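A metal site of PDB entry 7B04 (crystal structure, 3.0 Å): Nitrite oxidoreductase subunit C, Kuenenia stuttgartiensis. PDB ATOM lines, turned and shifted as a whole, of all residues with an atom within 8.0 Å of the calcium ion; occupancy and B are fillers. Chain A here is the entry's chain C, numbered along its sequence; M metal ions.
The side-chain carboxylate (OD2) of Asp 278 sits close to the side-chain hydroxyl (OG1) of Thr 273 (2.6 Å).
O of Asp 278 sits at hydrogen-bond distance from NE2 of Gln 280, 3.2 Å away.
The side-chain amide oxygen (OE1) of Gln 250 lies within hydrogen-bond range of the backbone NH (N) of Asp 235, at 3.1 Å.
The indole nitrogen (NE1) of Trp 165 sits close to the side-chain carboxylate (OD1) of Asp 235 (3.3 Å).
OE1 of Gln 247 sits close to OD2 of Asp 275 (2.9 Å).
NE2 of Gln 247 sits at hydrogen-bond distance from O of Leu 277 (3.2 Å).
The side-chain amide nitrogen (NE2) of Gln 247 sits close to the side-chain amide nitrogen (ND2) of Asn 163, at 3.3 Å.
NE2 of Gln 280 is in hydrogen-bond range of O of Asp 275 (3.4 Å).
Asp 275 touches the calcium ion (OD2 to CA, 3.2 Å).
Six residues have an atom within 4 Å of the calcium ion: Asp 235, Gln 247, His 249, Asp 251, Asp 275 and Asp 278.
The nearest printed residue that does not touch the calcium ion is Gln 250 (4.5 Å).
The calcium ion is bound by OD1 of Asp 278 (2.5 Å), OD2 of Asp 235 (2.5 Å), OE1 of Gln 247 (2.5 Å), O of His 249 (2.5 Å), OD1 of Asp 251 (2.6 Å) and OD2 of Asp 278 (2.7 Å).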
ATOM      1  N   ASN A 163       0.075  19.812  13.232  1.00  0.00           N
ATOM      2  CA  ASN A 163      -0.639  19.347  12.051  1.00  0.00           C
ATOM      3  C   ASN A 163      -2.108  19.754  12.174  1.00  0.00           C
ATOM      4  O   ASN A 163      -2.704  19.643  13.251  1.00  0.00           O
ATOM      5  CB  ASN A 163      -0.534  17.830  11.903  1.00  0.00           C
ATOM      6  CG  ASN A 163      -0.773  17.355  10.479  1.00  0.00           C
ATOM      7  OD1 ASN A 163      -0.533  16.191  10.156  1.00  0.00           O
ATOM      8  ND2 ASN A 163      -1.237  18.259   9.613  1.00  0.00           N
ATOM      9  N   LEU A 164      -2.677  20.221  11.071  1.00  0.00           N
ATOM     10  CA  LEU A 164      -4.053  20.704  11.036  1.00  0.00           C
ATOM     11  C   LEU A 164      -4.852  19.947   9.983  1.00  0.00           C
ATOM     12  O   LEU A 164      -4.334  19.660   8.899  1.00  0.00           O
ATOM     13  CB  LEU A 164      -4.112  22.205  10.713  1.00  0.00           C
ATOM     14  CG  LEU A 164      -3.802  23.336  11.706  1.00  0.00           C
ATOM     15  CD1 LEU A 164      -4.838  23.405  12.795  1.00  0.00           C
ATOM     16  CD2 LEU A 164      -2.400  23.216  12.283  1.00  0.00           C
ATOM     17  N   TRP A 165      -6.091  19.609  10.318  1.00  0.00           N
ATOM     18  CA  TRP A 165      -7.036  19.007   9.377  1.00  0.00           C
ATOM     19  C   TRP A 165      -8.242  19.942   9.284  1.00  0.00           C
ATOM     20  O   TRP A 165      -9.043  20.016  10.216  1.00  0.00           O
ATOM     21  CB  TRP A 165      -7.495  17.622   9.839  1.00  0.00           C
ATOM     22  CG  TRP A 165      -6.409  16.612   9.976  1.00  0.00           C
ATOM     23  CD1 TRP A 165      -5.115  16.717   9.551  1.00  0.00           C
ATOM     24  CD2 TRP A 165      -6.535  15.318  10.576  1.00  0.00           C
ATOM     25  NE1 TRP A 165      -4.425  15.564   9.865  1.00  0.00           N
ATOM     26  CE2 TRP A 165      -5.268  14.700  10.494  1.00  0.00           C
ATOM     27  CE3 TRP A 165      -7.581  14.628  11.192  1.00  0.00           C
ATOM     28  CZ2 TRP A 165      -5.037  13.411  10.993  1.00  0.00           C
ATOM     29  CZ3 TRP A 165      -7.345  13.359  11.681  1.00  0.00           C
ATOM     30  CH2 TRP A 165      -6.077  12.768  11.583  1.00  0.00           C
ATOM     31  N   ASP A 235      -5.087  19.181   4.427  1.00  0.00           N
ATOM     32  CA  ASP A 235      -4.028  18.760   5.336  1.00  0.00           C
ATOM     33  C   ASP A 235      -2.975  19.861   5.361  1.00  0.00           C
ATOM     34  O   ASP A 235      -2.392  20.177   4.320  1.00  0.00           O
ATOM     35  CB  ASP A 235      -3.434  17.429   4.881  1.00  0.00           C
ATOM     36  CG  ASP A 235      -2.499  16.831   5.913  1.00  0.00           C
ATOM     37  OD1 ASP A 235      -2.942  16.548   7.036  1.00  0.00           O
ATOM     38  OD2 ASP A 235      -1.320  16.610   5.568  1.00  0.00           O
ATOM     39  N   LEU A 236      -2.765  20.457   6.524  1.00  0.00           N
ATOM     40  CA  LEU A 236      -1.924  21.649   6.606  1.00  0.00           C
ATOM     41  C   LEU A 236      -1.239  21.714   7.962  1.00  0.00           C
ATOM     42  O   LEU A 236      -1.606  21.017   8.912  1.00  0.00           O
ATOM     43  CB  LEU A 236      -2.765  22.902   6.286  1.00  0.00           C
ATOM     44  CG  LEU A 236      -3.924  23.433   7.122  1.00  0.00           C
ATOM     45  CD1 LEU A 236      -4.475  24.646   6.396  1.00  0.00           C
ATOM     46  CD2 LEU A 236      -5.029  22.416   7.303  1.00  0.00           C
ATOM     47  N   ASN A 237      -0.208  22.570   8.054  1.00  0.00           N
ATOM     48  CA  ASN A 237       0.616  22.718   9.236  1.00  0.00           C
ATOM     49  C   ASN A 237       0.624  24.164   9.730  1.00  0.00           C
ATOM     50  O   ASN A 237       0.281  25.083   8.991  1.00  0.00           O
ATOM     51  CB  ASN A 237       2.068  22.286   8.968  1.00  0.00           C
ATOM     52  CG  ASN A 237       2.262  20.795   9.032  1.00  0.00           C
ATOM     53  OD1 ASN A 237       2.454  20.136   8.009  1.00  0.00           O
ATOM     54  ND2 ASN A 237       2.223  20.246  10.248  1.00  0.00           N
ATOM     55  N   GLN A 247      -0.018  22.165   3.204  1.00  0.00           N
ATOM     56  CA  GLN A 247       0.968  21.144   2.881  1.00  0.00           C
ATOM     57  C   GLN A 247       1.006  20.852   1.385  1.00  0.00           C
ATOM     58  O   GLN A 247       0.012  21.012   0.676  1.00  0.00           O
ATOM     59  CB  GLN A 247       0.689  19.847   3.634  1.00  0.00           C
ATOM     60  CG  GLN A 247       0.849  19.935   5.136  1.00  0.00           C
ATOM     61  CD  GLN A 247       0.985  18.570   5.771  1.00  0.00           C
ATOM     62  OE1 GLN A 247       1.138  17.566   5.076  1.00  0.00           O
ATOM     63  NE2 GLN A 247       0.922  18.519   7.090  1.00  0.00           N
ATOM     64  N   ASP A 248       2.177  20.419   0.917  1.00  0.00           N
ATOM     65  CA  ASP A 248       2.319  20.026  -0.479  1.00  0.00           C
ATOM     66  C   ASP A 248       1.643  18.679  -0.752  1.00  0.00           C
ATOM     67  O   ASP A 248       1.025  18.494  -1.803  1.00  0.00           O
ATOM     68  CB  ASP A 248       3.799  19.963  -0.848  1.00  0.00           C
ATOM     69  CG  ASP A 248       4.405  21.334  -1.055  1.00  0.00           C
ATOM     70  OD1 ASP A 248       3.978  22.053  -1.979  1.00  0.00           O
ATOM     71  OD2 ASP A 248       5.309  21.707  -0.272  1.00  0.00           O
ATOM     72  N   HIS A 249       1.760  17.739   0.174  1.00  0.00           N
ATOM     73  CA  HIS A 249       1.210  16.394   0.046  1.00  0.00           C
ATOM     74  C   HIS A 249      -0.004  16.272   0.957  1.00  0.00           C
ATOM     75  O   HIS A 249       0.144  16.194   2.185  1.00  0.00           O
ATOM     76  CB  HIS A 249       2.265  15.343   0.388  1.00  0.00           C
ATOM     77  CG  HIS A 249       1.911  13.962  -0.078  1.00  0.00           C
ATOM     78  ND1 HIS A 249       1.165  13.083   0.682  1.00  0.00           N
ATOM     79  CD2 HIS A 249       2.209  13.305  -1.229  1.00  0.00           C
ATOM     80  CE1 HIS A 249       1.011  11.947   0.020  1.00  0.00           C
ATOM     81  NE2 HIS A 249       1.637  12.060  -1.138  1.00  0.00           N
ATOM     82  N   GLN A 250      -1.196  16.255   0.372  1.00  0.00           N
ATOM     83  CA  GLN A 250      -2.438  16.202   1.143  1.00  0.00           C
ATOM     84  C   GLN A 250      -2.804  14.740   1.407  1.00  0.00           C
ATOM     85  O   GLN A 250      -2.862  13.928   0.474  1.00  0.00           O
ATOM     86  CB  GLN A 250      -3.579  16.887   0.399  1.00  0.00           C
ATOM     87  CG  GLN A 250      -3.216  18.235  -0.202  1.00  0.00           C
ATOM     88  CD  GLN A 250      -3.195  19.340   0.834  1.00  0.00           C
ATOM     89  OE1 GLN A 250      -4.193  19.613   1.490  1.00  0.00           O
ATOM     90  NE2 GLN A 250      -2.043  19.988   0.970  1.00  0.00           N
ATOM     91  N   ASP A 251      -3.059  14.419   2.673  1.00  0.00           N
ATOM     92  CA  ASP A 251      -3.276  13.038   3.083  1.00  0.00           C
ATOM     93  C   ASP A 251      -4.590  12.781   3.808  1.00  0.00           C
ATOM     94  O   ASP A 251      -4.982  11.624   3.927  1.00  0.00           O
ATOM     95  CB  ASP A 251      -2.124  12.576   3.990  1.00  0.00           C
ATOM     96  CG  ASP A 251      -0.876  12.225   3.212  1.00  0.00           C
ATOM     97  OD1 ASP A 251       0.202  12.780   3.527  1.00  0.00           O
ATOM     98  OD2 ASP A 251      -0.969  11.395   2.290  1.00  0.00           O
ATOM     99  N   VAL A 252      -5.272  13.813   4.291  1.00  0.00           N
ATOM    100  CA  VAL A 252      -6.522  13.646   5.034  1.00  0.00           C
ATOM    101  C   VAL A 252      -7.700  13.857   4.095  1.00  0.00           C
ATOM    102  O   VAL A 252      -7.647  14.716   3.199  1.00  0.00           O
ATOM    103  CB  VAL A 252      -6.580  14.596   6.248  1.00  0.00           C
ATOM    104  CG1 VAL A 252      -6.594  16.046   5.804  1.00  0.00           C
ATOM    105  CG2 VAL A 252      -7.795  14.283   7.116  1.00  0.00           C
ATOM    106  N   ARG A 269      -8.045   9.500   7.767  1.00  0.00           N
ATOM    107  CA  ARG A 269      -6.621   9.549   7.486  1.00  0.00           C
ATOM    108  C   ARG A 269      -6.011   8.216   7.866  1.00  0.00           C
ATOM    109  O   ARG A 269      -6.474   7.559   8.796  1.00  0.00           O
ATOM    110  CB  ARG A 269      -5.946  10.680   8.278  1.00  0.00           C
ATOM    111  CG  ARG A 269      -4.916  11.526   7.542  1.00  0.00           C
ATOM    112  CD  ARG A 269      -3.523  10.902   7.461  1.00  0.00           C
ATOM    113  NE  ARG A 269      -3.009  10.392   8.737  1.00  0.00           N
ATOM    114  CZ  ARG A 269      -2.282  11.104   9.599  1.00  0.00           C
ATOM    115  NH1 ARG A 269      -1.843  10.544  10.721  1.00  0.00           N
ATOM    116  NH2 ARG A 269      -2.002  12.383   9.357  1.00  0.00           N
ATOM    117  N   THR A 273       1.687   7.982   7.534  1.00  0.00           N
ATOM    118  CA  THR A 273       1.828   8.545   6.193  1.00  0.00           C
ATOM    119  C   THR A 273       3.308   8.798   5.925  1.00  0.00           C
ATOM    120  O   THR A 273       4.103   8.984   6.846  1.00  0.00           O
ATOM    121  CB  THR A 273       1.049   9.854   6.024  1.00  0.00           C
ATOM    122  OG1 THR A 273       1.501  10.812   6.984  1.00  0.00           O
ATOM    123  CG2 THR A 273      -0.436   9.617   6.216  1.00  0.00           C
ATOM    124  N   GLY A 274       3.665   8.821   4.638  1.00  0.00           N
ATOM    125  CA  GLY A 274       5.040   9.077   4.243  1.00  0.00           C
ATOM    126  C   GLY A 274       5.496  10.519   4.389  1.00  0.00           C
ATOM    127  O   GLY A 274       6.685  10.786   4.151  1.00  0.00           O
ATOM    128  N   ASP A 275       4.617  11.444   4.775  1.00  0.00           N
ATOM    129  CA  ASP A 275       5.017  12.845   4.966  1.00  0.00           C
ATOM    130  C   ASP A 275       5.513  13.039   6.392  1.00  0.00           C
ATOM    131  O   ASP A 275       4.765  12.781   7.335  1.00  0.00           O
ATOM    132  CB  ASP A 275       3.859  13.798   4.680  1.00  0.00           C
ATOM    133  CG  ASP A 275       4.225  15.293   4.935  1.00  0.00           C
ATOM    134  OD1 ASP A 275       5.141  15.621   5.719  1.00  0.00           O
ATOM    135  OD2 ASP A 275       3.571  16.144   4.307  1.00  0.00           O
ATOM    136  N   PRO A 276       6.755  13.490   6.589  1.00  0.00           N
ATOM    137  CA  PRO A 276       7.244  13.722   7.959  1.00  0.00           C
ATOM    138  C   PRO A 276       6.521  14.855   8.673  1.00  0.00           C
ATOM    139  O   PRO A 276       6.559  14.888   9.910  1.00  0.00           O
ATOM    140  CB  PRO A 276       8.730  14.065   7.743  1.00  0.00           C
ATOM    141  CG  PRO A 276       9.055  13.535   6.373  1.00  0.00           C
ATOM    142  CD  PRO A 276       7.801  13.679   5.575  1.00  0.00           C
ATOM    143  N   LEU A 277       5.879  15.772   7.963  1.00  0.00           N
ATOM    144  CA  LEU A 277       5.129  16.869   8.583  1.00  0.00           C
ATOM    145  C   LEU A 277       3.725  16.434   8.974  1.00  0.00           C
ATOM    146  O   LEU A 277       2.894  17.297   9.302  1.00  0.00           O
ATOM    147  CB  LEU A 277       5.057  18.078   7.645  1.00  0.00           C
ATOM    148  CG  LEU A 277       6.359  18.787   7.299  1.00  0.00           C
ATOM    149  CD1 LEU A 277       6.113  19.895   6.282  1.00  0.00           C
ATOM    150  CD2 LEU A 277       7.035  19.327   8.553  1.00  0.00           C
ATOM    151  N   ASP A 278       3.439  15.139   8.950  1.00  0.00           N
ATOM    152  CA  ASP A 278       2.141  14.598   9.317  1.00  0.00           C
ATOM    153  C   ASP A 278       2.211  14.020  10.719  1.00  0.00           C
ATOM    154  O   ASP A 278       3.235  13.465  11.120  1.00  0.00           O
ATOM    155  CB  ASP A 278       1.721  13.500   8.343  1.00  0.00           C
ATOM    156  CG  ASP A 278       1.059  14.033   7.091  1.00  0.00           C
ATOM    157  OD1 ASP A 278       0.929  15.266   6.951  1.00  0.00           O
ATOM    158  OD2 ASP A 278       0.684  13.203   6.231  1.00  0.00           O
ATOM    159  N   VAL A 279       1.108  14.144  11.470  1.00  0.00           N
ATOM    160  CA  VAL A 279       1.027  13.479  12.762  1.00  0.00           C
ATOM    161  C   VAL A 279       1.046  11.967  12.544  1.00  0.00           C
ATOM    162  O   VAL A 279       0.425  11.451  11.607  1.00  0.00           O
ATOM    163  CB  VAL A 279      -0.208  13.944  13.545  1.00  0.00           C
ATOM    164  CG1 VAL A 279      -1.490  13.320  13.010  1.00  0.00           C
ATOM    165  CG2 VAL A 279      -0.032  13.625  15.031  1.00  0.00           C
ATOM    166  N   GLN A 280       1.791  11.262  13.387  1.00  0.00           N
ATOM    167  CA  GLN A 280       1.929   9.810  13.293  1.00  0.00           C
ATOM    168  C   GLN A 280       1.269   9.155  14.499  1.00  0.00           C
ATOM    169  O   GLN A 280       1.692   9.380  15.635  1.00  0.00           O
ATOM    170  CB  GLN A 280       3.398   9.413  13.188  1.00  0.00           C
ATOM    171  CG  GLN A 280       4.150  10.064  12.028  1.00  0.00           C
ATOM    172  CD  GLN A 280       3.582   9.664  10.683  1.00  0.00           C
ATOM    173  OE1 GLN A 280       3.145   8.531  10.481  1.00  0.00           O
ATOM    174  NE2 GLN A 280       3.597  10.605   9.742  1.00  0.00           N
HETATM  175 CA    CA M   1       0.467  15.208   4.491  1.00  0.00          CA
